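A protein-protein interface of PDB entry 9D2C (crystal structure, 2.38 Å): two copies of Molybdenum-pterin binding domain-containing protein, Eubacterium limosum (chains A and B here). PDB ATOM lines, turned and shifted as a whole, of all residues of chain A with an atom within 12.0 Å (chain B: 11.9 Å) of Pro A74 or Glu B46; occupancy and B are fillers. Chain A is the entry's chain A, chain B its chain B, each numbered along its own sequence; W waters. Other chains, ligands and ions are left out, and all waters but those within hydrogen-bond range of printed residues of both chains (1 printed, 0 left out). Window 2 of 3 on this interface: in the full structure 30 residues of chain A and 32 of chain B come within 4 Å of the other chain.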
ATOM      1  N   ILE A  66       6.266 -19.925  -9.899  1.00  0.00           N
ATOM      2  CA  ILE A  66       6.708 -20.383 -11.203  1.00  0.00           C
ATOM      3  C   ILE A  66       7.002 -19.166 -12.048  1.00  0.00           C
ATOM      4  O   ILE A  66       6.236 -18.198 -12.035  1.00  0.00           O
ATOM      5  CB  ILE A  66       5.676 -21.281 -11.908  1.00  0.00           C
ATOM      6  CG1 ILE A  66       5.493 -22.578 -11.121  1.00  0.00           C
ATOM      7  CG2 ILE A  66       6.126 -21.538 -13.313  1.00  0.00           C
ATOM      8  CD1 ILE A  66       6.736 -23.452 -11.111  1.00  0.00           C
ATOM      9  N   GLY A  67       8.119 -19.211 -12.771  1.00  0.00           N
ATOM     10  CA  GLY A  67       8.444 -18.164 -13.719  1.00  0.00           C
ATOM     11  C   GLY A  67       8.644 -18.713 -15.119  1.00  0.00           C
ATOM     12  O   GLY A  67       8.878 -19.912 -15.297  1.00  0.00           O
ATOM     13  N   ILE A  68       8.546 -17.841 -16.123  1.00  0.00           N
ATOM     14  CA  ILE A  68       8.778 -18.195 -17.519  1.00  0.00           C
ATOM     15  C   ILE A  68       9.530 -17.043 -18.175  1.00  0.00           C
ATOM     16  O   ILE A  68       9.542 -15.913 -17.681  1.00  0.00           O
ATOM     17  CB  ILE A  68       7.472 -18.520 -18.292  1.00  0.00           C
ATOM     18  CG1 ILE A  68       6.517 -17.322 -18.305  1.00  0.00           C
ATOM     19  CG2 ILE A  68       6.776 -19.753 -17.725  1.00  0.00           C
ATOM     20  CD1 ILE A  68       5.293 -17.553 -19.158  1.00  0.00           C
ATOM     21  N   ASP A  69      10.148 -17.336 -19.308  1.00  0.00           N
ATOM     22  CA  ASP A  69      10.865 -16.298 -20.029  1.00  0.00           C
ATOM     23  C   ASP A  69       9.905 -15.245 -20.574  1.00  0.00           C
ATOM     24  O   ASP A  69       8.752 -15.532 -20.909  1.00  0.00           O
ATOM     25  CB  ASP A  69      11.691 -16.932 -21.146  1.00  0.00           C
ATOM     26  CG  ASP A  69      12.820 -17.802 -20.605  1.00  0.00           C
ATOM     27  OD1 ASP A  69      13.433 -17.429 -19.580  1.00  0.00           O
ATOM     28  OD2 ASP A  69      13.095 -18.866 -21.189  1.00  0.00           O
ATOM     29  N   ASP A  70      10.387 -13.996 -20.605  1.00  0.00           N
ATOM     30  CA  ASP A  70       9.566 -12.887 -21.080  1.00  0.00           C
ATOM     31  C   ASP A  70       9.084 -13.116 -22.507  1.00  0.00           C
ATOM     32  O   ASP A  70       8.027 -12.602 -22.890  1.00  0.00           O
ATOM     33  CB  ASP A  70      10.347 -11.566 -21.037  1.00  0.00           C
ATOM     34  CG  ASP A  70      10.618 -11.063 -19.630  1.00  0.00           C
ATOM     35  OD1 ASP A  70       9.665 -10.614 -18.950  1.00  0.00           O
ATOM     36  OD2 ASP A  70      11.798 -11.095 -19.218  1.00  0.00           O
ATOM     37  N   TRP A  71       9.865 -13.832 -23.326  1.00  0.00           N
ATOM     38  CA  TRP A  71       9.499 -14.054 -24.727  1.00  0.00           C
ATOM     39  C   TRP A  71       8.603 -15.277 -24.837  1.00  0.00           C
ATOM     40  O   TRP A  71       8.714 -16.049 -25.794  1.00  0.00           O
ATOM     41  CB  TRP A  71      10.722 -14.246 -25.645  1.00  0.00           C
ATOM     42  CG  TRP A  71      11.630 -15.361 -25.220  1.00  0.00           C
ATOM     43  CD1 TRP A  71      11.560 -16.669 -25.603  1.00  0.00           C
ATOM     44  CD2 TRP A  71      12.754 -15.262 -24.313  1.00  0.00           C
ATOM     45  NE1 TRP A  71      12.564 -17.393 -24.992  1.00  0.00           N
ATOM     46  CE2 TRP A  71      13.310 -16.556 -24.196  1.00  0.00           C
ATOM     47  CE3 TRP A  71      13.338 -14.205 -23.588  1.00  0.00           C
ATOM     48  CZ2 TRP A  71      14.436 -16.828 -23.377  1.00  0.00           C
ATOM     49  CZ3 TRP A  71      14.462 -14.477 -22.770  1.00  0.00           C
ATOM     50  CH2 TRP A  71      14.992 -15.777 -22.680  1.00  0.00           C
ATOM     51  N   SER A  72       7.774 -15.499 -23.825  1.00  0.00           N
ATOM     52  CA  SER A  72       6.704 -16.488 -23.873  1.00  0.00           C
ATOM     53  C   SER A  72       5.394 -15.718 -23.834  1.00  0.00           C
ATOM     54  O   SER A  72       5.217 -14.836 -22.984  1.00  0.00           O
ATOM     55  CB  SER A  72       6.777 -17.487 -22.709  1.00  0.00           C
ATOM     56  OG  SER A  72       5.807 -18.523 -22.859  1.00  0.00           O
ATOM     57  N   HIS A  73       4.496 -16.021 -24.774  1.00  0.00           N
ATOM     58  CA  HIS A  73       3.217 -15.329 -24.901  1.00  0.00           C
ATOM     59  C   HIS A  73       2.077 -16.323 -24.731  1.00  0.00           C
ATOM     60  O   HIS A  73       1.368 -16.640 -25.696  1.00  0.00           O
ATOM     61  CB  HIS A  73       3.106 -14.622 -26.244  1.00  0.00           C
ATOM     62  CG  HIS A  73       4.407 -14.075 -26.716  1.00  0.00           C
ATOM     63  ND1 HIS A  73       4.897 -12.874 -26.273  1.00  0.00           N
ATOM     64  CD2 HIS A  73       5.332 -14.594 -27.556  1.00  0.00           C
ATOM     65  CE1 HIS A  73       6.073 -12.656 -26.843  1.00  0.00           C
ATOM     66  NE2 HIS A  73       6.356 -13.680 -27.621  1.00  0.00           N
ATOM     67  N   PRO A  74       1.885 -16.848 -23.508  1.00  0.00           N
ATOM     68  CA  PRO A  74       0.630 -17.521 -23.150  1.00  0.00           C
ATOM     69  C   PRO A  74      -0.594 -16.674 -23.537  1.00  0.00           C
ATOM     70  O   PRO A  74      -0.674 -15.459 -23.308  1.00  0.00           O
ATOM     71  CB  PRO A  74       0.736 -17.689 -21.626  1.00  0.00           C
ATOM     72  CG  PRO A  74       1.888 -16.753 -21.177  1.00  0.00           C
ATOM     73  CD  PRO A  74       2.809 -16.738 -22.361  1.00  0.00           C
ATOM     74  N   VAL B  13       8.156 -28.499 -16.964  1.00  0.00           N
ATOM     75  CA  VAL B  13       6.952 -28.946 -16.271  1.00  0.00           C
ATOM     76  C   VAL B  13       6.743 -30.433 -16.525  1.00  0.00           C
ATOM     77  O   VAL B  13       6.695 -30.878 -17.688  1.00  0.00           O
ATOM     78  CB  VAL B  13       5.740 -28.115 -16.722  1.00  0.00           C
ATOM     79  CG1 VAL B  13       4.475 -28.641 -16.103  1.00  0.00           C
ATOM     80  CG2 VAL B  13       5.940 -26.631 -16.395  1.00  0.00           C
ATOM     81  N   ILE B  16       0.908 -31.174 -13.811  1.00  0.00           N
ATOM     82  CA  ILE B  16       0.045 -30.081 -13.400  1.00  0.00           C
ATOM     83  C   ILE B  16      -1.222 -30.717 -12.842  1.00  0.00           C
ATOM     84  O   ILE B  16      -1.975 -31.349 -13.581  1.00  0.00           O
ATOM     85  CB  ILE B  16      -0.305 -29.116 -14.540  1.00  0.00           C
ATOM     86  CG1 ILE B  16       0.950 -28.404 -15.036  1.00  0.00           C
ATOM     87  CG2 ILE B  16      -1.353 -28.106 -14.099  1.00  0.00           C
ATOM     88  CD1 ILE B  16       0.741 -27.571 -16.288  1.00  0.00           C
ATOM     89  N   GLU B  18      -4.576 -29.492 -11.431  1.00  0.00           N
ATOM     90  CA  GLU B  18      -5.434 -28.331 -11.322  1.00  0.00           C
ATOM     91  C   GLU B  18      -6.375 -28.516 -10.140  1.00  0.00           C
ATOM     92  O   GLU B  18      -6.860 -29.619  -9.879  1.00  0.00           O
ATOM     93  CB  GLU B  18      -6.196 -28.102 -12.628  1.00  0.00           C
ATOM     94  CG  GLU B  18      -5.275 -28.061 -13.840  1.00  0.00           C
ATOM     95  CD  GLU B  18      -5.839 -27.206 -14.968  1.00  0.00           C
ATOM     96  OE1 GLU B  18      -5.032 -26.599 -15.716  1.00  0.00           O
ATOM     97  OE2 GLU B  18      -7.074 -27.164 -15.148  1.00  0.00           O
ATOM     98  N   VAL B  21      -8.974 -22.996  -6.626  1.00  0.00           N
ATOM     99  CA  VAL B  21      -8.352 -21.693  -6.818  1.00  0.00           C
ATOM    100  C   VAL B  21      -6.838 -21.792  -6.954  1.00  0.00           C
ATOM    101  O   VAL B  21      -6.206 -20.805  -7.349  1.00  0.00           O
ATOM    102  CB  VAL B  21      -8.727 -20.719  -5.682  1.00  0.00           C
ATOM    103  CG1 VAL B  21     -10.239 -20.430  -5.698  1.00  0.00           C
ATOM    104  CG2 VAL B  21      -8.269 -21.279  -4.338  1.00  0.00           C
ATOM    105  N   ASN B  22      -6.236 -22.919  -6.579  1.00  0.00           N
ATOM    106  CA  ASN B  22      -4.814 -23.176  -6.744  1.00  0.00           C
ATOM    107  C   ASN B  22      -4.605 -24.426  -7.589  1.00  0.00           C
ATOM    108  O   ASN B  22      -5.528 -25.201  -7.845  1.00  0.00           O
ATOM    109  CB  ASN B  22      -4.106 -23.376  -5.393  1.00  0.00           C
ATOM    110  CG  ASN B  22      -4.050 -22.111  -4.561  1.00  0.00           C
ATOM    111  OD1 ASN B  22      -3.524 -21.082  -4.997  1.00  0.00           O
ATOM    112  ND2 ASN B  22      -4.603 -22.177  -3.355  1.00  0.00           N
ATOM    113  N   GLY B  23      -3.376 -24.584  -8.059  1.00  0.00           N
ATOM    114  CA  GLY B  23      -2.928 -25.825  -8.638  1.00  0.00           C
ATOM    115  C   GLY B  23      -1.499 -26.074  -8.199  1.00  0.00           C
ATOM    116  O   GLY B  23      -0.851 -25.202  -7.604  1.00  0.00           O
ATOM    117  N   VAL B  25       2.170 -27.337  -9.651  1.00  0.00           N
ATOM    118  CA  VAL B  25       3.034 -27.539 -10.807  1.00  0.00           C
ATOM    119  C   VAL B  25       4.320 -28.190 -10.325  1.00  0.00           C
ATOM    120  O   VAL B  25       4.967 -27.678  -9.407  1.00  0.00           O
ATOM    121  CB  VAL B  25       3.332 -26.200 -11.499  1.00  0.00           C
ATOM    122  CG1 VAL B  25       4.138 -26.425 -12.791  1.00  0.00           C
ATOM    123  CG2 VAL B  25       2.021 -25.424 -11.701  1.00  0.00           C
ATOM    124  N   ILE B  39       0.444 -22.781  -6.541  1.00  0.00           N
ATOM    125  CA  ILE B  39       0.186 -21.414  -6.985  1.00  0.00           C
ATOM    126  C   ILE B  39      -1.263 -21.342  -7.427  1.00  0.00           C
ATOM    127  O   ILE B  39      -1.953 -22.348  -7.479  1.00  0.00           O
ATOM    128  CB  ILE B  39       1.141 -20.990  -8.121  1.00  0.00           C
ATOM    129  CG1 ILE B  39       1.146 -22.054  -9.230  1.00  0.00           C
ATOM    130  CG2 ILE B  39       2.511 -20.740  -7.530  1.00  0.00           C
ATOM    131  CD1 ILE B  39       1.900 -21.640 -10.503  1.00  0.00           C
ATOM    132  N   SER B  40      -1.727 -20.137  -7.737  1.00  0.00           N
ATOM    133  CA  SER B  40      -3.127 -19.958  -8.108  1.00  0.00           C
ATOM    134  C   SER B  40      -3.414 -20.493  -9.511  1.00  0.00           C
ATOM    135  O   SER B  40      -2.565 -20.454 -10.406  1.00  0.00           O
ATOM    136  CB  SER B  40      -3.510 -18.480  -8.064  1.00  0.00           C
ATOM    137  OG  SER B  40      -2.920 -17.798  -9.157  1.00  0.00           O
ATOM    138  N   MET B  41      -4.639 -20.989  -9.704  1.00  0.00           N
ATOM    139  CA  MET B  41      -5.053 -21.386 -11.045  1.00  0.00           C
ATOM    140  C   MET B  41      -4.955 -20.219 -12.018  1.00  0.00           C
ATOM    141  O   MET B  41      -4.585 -20.406 -13.183  1.00  0.00           O
ATOM    142  CB  MET B  41      -6.479 -21.944 -11.041  1.00  0.00           C
ATOM    143  CG  MET B  41      -6.616 -23.285 -10.354  1.00  0.00           C
ATOM    144  SD  MET B  41      -5.636 -24.593 -11.149  1.00  0.00           S
ATOM    145  CE  MET B  41      -5.835 -24.225 -12.903  1.00  0.00           C
ATOM    146  N   ASP B  42      -5.259 -19.004 -11.561  1.00  0.00           N
ATOM    147  CA  ASP B  42      -5.114 -17.858 -12.446  1.00  0.00           C
ATOM    148  C   ASP B  42      -3.700 -17.820 -13.026  1.00  0.00           C
ATOM    149  O   ASP B  42      -3.518 -17.716 -14.237  1.00  0.00           O
ATOM    150  CB  ASP B  42      -5.425 -16.556 -11.699  1.00  0.00           C
ATOM    151  CG  ASP B  42      -6.895 -16.397 -11.375  1.00  0.00           C
ATOM    152  OD1 ASP B  42      -7.730 -16.536 -12.298  1.00  0.00           O
ATOM    153  OD2 ASP B  42      -7.213 -16.144 -10.183  1.00  0.00           O
ATOM    154  N   SER B  43      -2.682 -18.003 -12.190  1.00  0.00           N
ATOM    155  CA  SER B  43      -1.323 -17.909 -12.713  1.00  0.00           C
ATOM    156  C   SER B  43      -0.960 -19.100 -13.588  1.00  0.00           C
ATOM    157  O   SER B  43      -0.227 -18.956 -14.572  1.00  0.00           O
ATOM    158  CB  SER B  43      -0.323 -17.787 -11.570  1.00  0.00           C
ATOM    159  OG  SER B  43      -0.423 -16.511 -10.975  1.00  0.00           O
ATOM    160  N   ILE B  44      -1.419 -20.291 -13.233  1.00  0.00           N
ATOM    161  CA  ILE B  44      -1.133 -21.436 -14.087  1.00  0.00           C
ATOM    162  C   ILE B  44      -1.672 -21.176 -15.487  1.00  0.00           C
ATOM    163  O   ILE B  44      -1.051 -21.538 -16.493  1.00  0.00           O
ATOM    164  CB  ILE B  44      -1.707 -22.720 -13.464  1.00  0.00           C
ATOM    165  CG1 ILE B  44      -0.937 -23.053 -12.181  1.00  0.00           C
ATOM    166  CG2 ILE B  44      -1.637 -23.846 -14.459  1.00  0.00           C
ATOM    167  CD1 ILE B  44      -1.552 -24.161 -11.345  1.00  0.00           C
ATOM    168  N   ARG B  45      -2.842 -20.548 -15.569  1.00  0.00           N
ATOM    169  CA  ARG B  45      -3.442 -20.237 -16.862  1.00  0.00           C
ATOM    170  C   ARG B  45      -2.720 -19.101 -17.580  1.00  0.00           C
ATOM    171  O   ARG B  45      -2.351 -19.235 -18.750  1.00  0.00           O
ATOM    172  CB  ARG B  45      -4.909 -19.878 -16.652  1.00  0.00           C
ATOM    173  CG  ARG B  45      -5.706 -21.025 -16.107  1.00  0.00           C
ATOM    174  CD  ARG B  45      -7.174 -20.741 -16.113  1.00  0.00           C
ATOM    175  NE  ARG B  45      -7.908 -21.938 -15.731  1.00  0.00           N
ATOM    176  CZ  ARG B  45      -9.012 -21.937 -15.002  1.00  0.00           C
ATOM    177  NH1 ARG B  45      -9.533 -20.811 -14.542  1.00  0.00           N
ATOM    178  NH2 ARG B  45      -9.611 -23.092 -14.737  1.00  0.00           N
ATOM    179  N   GLU B  46      -2.513 -17.972 -16.900  1.00  0.00           N
ATOM    180  CA  GLU B  46      -1.950 -16.806 -17.572  1.00  0.00           C
ATOM    181  C   GLU B  46      -0.540 -17.063 -18.077  1.00  0.00           C
ATOM    182  O   GLU B  46      -0.146 -16.519 -19.112  1.00  0.00           O
ATOM    183  CB  GLU B  46      -1.950 -15.593 -16.645  1.00  0.00           C
ATOM    184  CG  GLU B  46      -3.284 -15.364 -15.960  1.00  0.00           C
ATOM    185  CD  GLU B  46      -3.371 -14.021 -15.252  1.00  0.00           C
ATOM    186  OE1 GLU B  46      -2.326 -13.348 -15.132  1.00  0.00           O
ATOM    187  OE2 GLU B  46      -4.493 -13.632 -14.850  1.00  0.00           O
ATOM    188  N   LEU B  47       0.239 -17.861 -17.353  1.00  0.00           N
ATOM    189  CA  LEU B  47       1.576 -18.239 -17.792  1.00  0.00           C
ATOM    190  C   LEU B  47       1.561 -19.316 -18.870  1.00  0.00           C
ATOM    191  O   LEU B  47       2.625 -19.632 -19.413  1.00  0.00           O
ATOM    192  CB  LEU B  47       2.390 -18.755 -16.602  1.00  0.00           C
ATOM    193  CG  LEU B  47       2.664 -17.769 -15.473  1.00  0.00           C
ATOM    194  CD1 LEU B  47       3.533 -18.357 -14.387  1.00  0.00           C
ATOM    195  CD2 LEU B  47       3.330 -16.532 -16.061  1.00  0.00           C
ATOM    196  N   GLY B  48       0.391 -19.871 -19.199  1.00  0.00           N
ATOM    197  CA  GLY B  48       0.289 -20.883 -20.243  1.00  0.00           C
ATOM    198  C   GLY B  48       0.984 -22.178 -19.911  1.00  0.00           C
ATOM    199  O   GLY B  48       1.371 -22.930 -20.806  1.00  0.00           O
ATOM    200  N   LEU B  49       1.109 -22.489 -18.640  1.00  0.00           N
ATOM    201  CA  LEU B  49       1.857 -23.670 -18.273  1.00  0.00           C
ATOM    202  C   LEU B  49       1.157 -24.956 -18.726  1.00  0.00           C
ATOM    203  O   LEU B  49      -0.051 -25.137 -18.520  1.00  0.00           O
ATOM    204  CB  LEU B  49       2.075 -23.616 -16.763  1.00  0.00           C
ATOM    205  CG  LEU B  49       2.941 -22.543 -16.065  1.00  0.00           C
ATOM    206  CD1 LEU B  49       2.776 -22.840 -14.554  1.00  0.00           C
ATOM    207  CD2 LEU B  49       4.381 -22.607 -16.537  1.00  0.00           C
ATOM    208  N   GLN B  50       1.910 -25.800 -19.449  1.00  0.00           N
ATOM    209  CA  GLN B  50       1.496 -27.179 -19.646  1.00  0.00           C
ATOM    210  C   GLN B  50       2.724 -28.079 -19.598  1.00  0.00           C
ATOM    211  O   GLN B  50       3.870 -27.630 -19.426  1.00  0.00           O
ATOM    212  CB  GLN B  50       0.711 -27.404 -20.926  1.00  0.00           C
ATOM    213  CG  GLN B  50      -0.506 -26.491 -21.037  1.00  0.00           C
ATOM    214  CD  GLN B  50      -1.236 -26.626 -22.365  1.00  0.00           C
ATOM    215  OE1 GLN B  50      -0.642 -27.031 -23.372  1.00  0.00           O
ATOM    216  NE2 GLN B  50      -2.565 -26.443 -22.333  1.00  0.00           N
ATOM    217  N   SER B  53       6.456 -27.399 -20.617  1.00  0.00           N
ATOM    218  CA  SER B  53       6.841 -25.995 -20.678  1.00  0.00           C
ATOM    219  C   SER B  53       8.148 -25.776 -19.932  1.00  0.00           C
ATOM    220  O   SER B  53       8.410 -26.391 -18.895  1.00  0.00           O
ATOM    221  CB  SER B  53       5.747 -25.110 -20.082  1.00  0.00           C
ATOM    222  OG  SER B  53       4.532 -25.235 -20.808  1.00  0.00           O
ATOM    223  N   ASP B  54       8.979 -24.910 -20.485  1.00  0.00           N
ATOM    224  CA  ASP B  54      10.171 -24.444 -19.799  1.00  0.00           C
ATOM    225  C   ASP B  54       9.745 -23.382 -18.799  1.00  0.00           C
ATOM    226  O   ASP B  54       8.909 -22.532 -19.112  1.00  0.00           O
ATOM    227  CB  ASP B  54      11.172 -23.902 -20.822  1.00  0.00           C
ATOM    228  CG  ASP B  54      11.724 -25.006 -21.744  1.00  0.00           C
ATOM    229  OD1 ASP B  54      12.257 -25.998 -21.230  1.00  0.00           O
ATOM    230  OD2 ASP B  54      11.571 -24.913 -22.975  1.00  0.00           O
ATOM    231  N   ALA B  55      10.271 -23.463 -17.583  1.00  0.00           N
ATOM    232  CA  ALA B  55       9.913 -22.514 -16.542  1.00  0.00           C
ATOM    233  C   ALA B  55      11.049 -22.425 -15.530  1.00  0.00           C
ATOM    234  O   ALA B  55      12.096 -23.061 -15.681  1.00  0.00           O
ATOM    235  CB  ALA B  55       8.612 -22.919 -15.837  1.00  0.00           C
ATOM    236  N   TYR B  56      10.810 -21.640 -14.473  1.00  0.00           N
ATOM    237  CA  TYR B  56      11.733 -21.470 -13.360  1.00  0.00           C
ATOM    238  C   TYR B  56      10.934 -21.642 -12.073  1.00  0.00           C
ATOM    239  O   TYR B  56       9.840 -21.091 -11.938  1.00  0.00           O
ATOM    240  CB  TYR B  56      12.424 -20.066 -13.389  1.00  0.00           C
ATOM    241  CG  TYR B  56      13.136 -19.770 -14.698  1.00  0.00           C
ATOM    242  CD1 TYR B  56      12.412 -19.401 -15.819  1.00  0.00           C
ATOM    243  CD2 TYR B  56      14.515 -19.873 -14.817  1.00  0.00           C
ATOM    244  CE1 TYR B  56      13.024 -19.151 -17.014  1.00  0.00           C
ATOM    245  CE2 TYR B  56      15.140 -19.629 -16.020  1.00  0.00           C
ATOM    246  CZ  TYR B  56      14.383 -19.260 -17.115  1.00  0.00           C
ATOM    247  OH  TYR B  56      14.964 -19.003 -18.333  1.00  0.00           O
HETATM  248  O   HOH W   1      10.360 -20.192 -20.176  1.00  0.00           O
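N of Gly A67 is in hydrogen-bond range of O of Tyr B56 (2.7 Å). The side-chain carboxylate of Asp A69 lies within hydrogen-bond range of the side-chain hydroxyl of Tyr B56, 2.5 Å away.
Ile B39 touches Ile A66. Leu B47 touches Ile A66 (CD1 to O, 3.6 Å). Leu B49 touches Ile A66 (CD1 to CG2, 3.8 Å). CG2 of Ile A66 touches CB of Ala B55, 3.8 Å away. CA of Ile A66 touches O of Tyr B56, 3.3 Å away. CA of Ala B55 touches O of Gly A67, at 3.1 Å. Asp B54 touches Ile A68. Glu B46 touches Pro A74. Pro A74 touches Leu B47 (CB to C, 3.3 Å). Pro A74 touches Gly B48 (CB to N, 3.3 Å).
No position is printed for both chains. Of the 14 pairs that touch across the chains among the printed residues, none has its exchanged pair printed and touching as well.
Printed residues of chain B within 4 Å of Ile A68: Leu B47, Leu B49 and Asp B54. Printed residues of chain B within 4 Å of Asp A69: Tyr B56 (2.5 Å). Pro A74 touches just these residues of chain B: Glu B46, Leu B47 and Gly B48. Glu B18 touches none of the printed residues of chain A. Printed residues of chain A within 4 Å of Ile B39: Ile A66. Asp B42 touches none of the printed residues of chain A. No residue of chain A comes within 4 Å of Ser B43. Leu B47 touches just these residues of chain A: Ile A66 (3.6 Å), Ile A68 (3.4 Å) and Pro A74 (3.3 Å). Of chain A, only Pro A74 comes within 4 Å of Gly B48. The nearest residue of chain B that does not touch Pro A74 is Arg B45 (4.5 Å). The nearest residue of chain A that does not touch Glu B46 is Ile A68 (5.5 Å). The nearest printed residue of chain B that does not touch Asp A69 is Asp B54 (5.3 Å).
The backbone carbonyl oxygen of Ile B39 lies close to the side-chain amide oxygen of Asn B22, 3.2 Å away. The backbone NH (N) of Gly B23 is in hydrogen-bond range of the backbone carbonyl oxygen (O) of Ile B39. O of Ile B44 is in hydrogen-bond range of N of Leu B49, at 3.2 Å.
Water W1 bridges O of Asp B54 (3.0 Å) and N of Asp A69 (3.0 Å).
Hydrophobic or aromatic side chains of chain A that line the printed part of chain B: Ile A66, Ile A68 and Pro A74. Printed residues of chain B that touch a printed residue of chain A: Ile B39, Glu B46, Leu B47, Gly B48, Leu B49, Asp B54, Ala B55 and Tyr B56. Hydrophobic or aromatic side chains of chain B within 4 Å of the printed part of chain A: Ile B39, Leu B47, Leu B49, Ala B55 and Tyr B56. Among the printed residues, 14 pairs touch across the chains.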
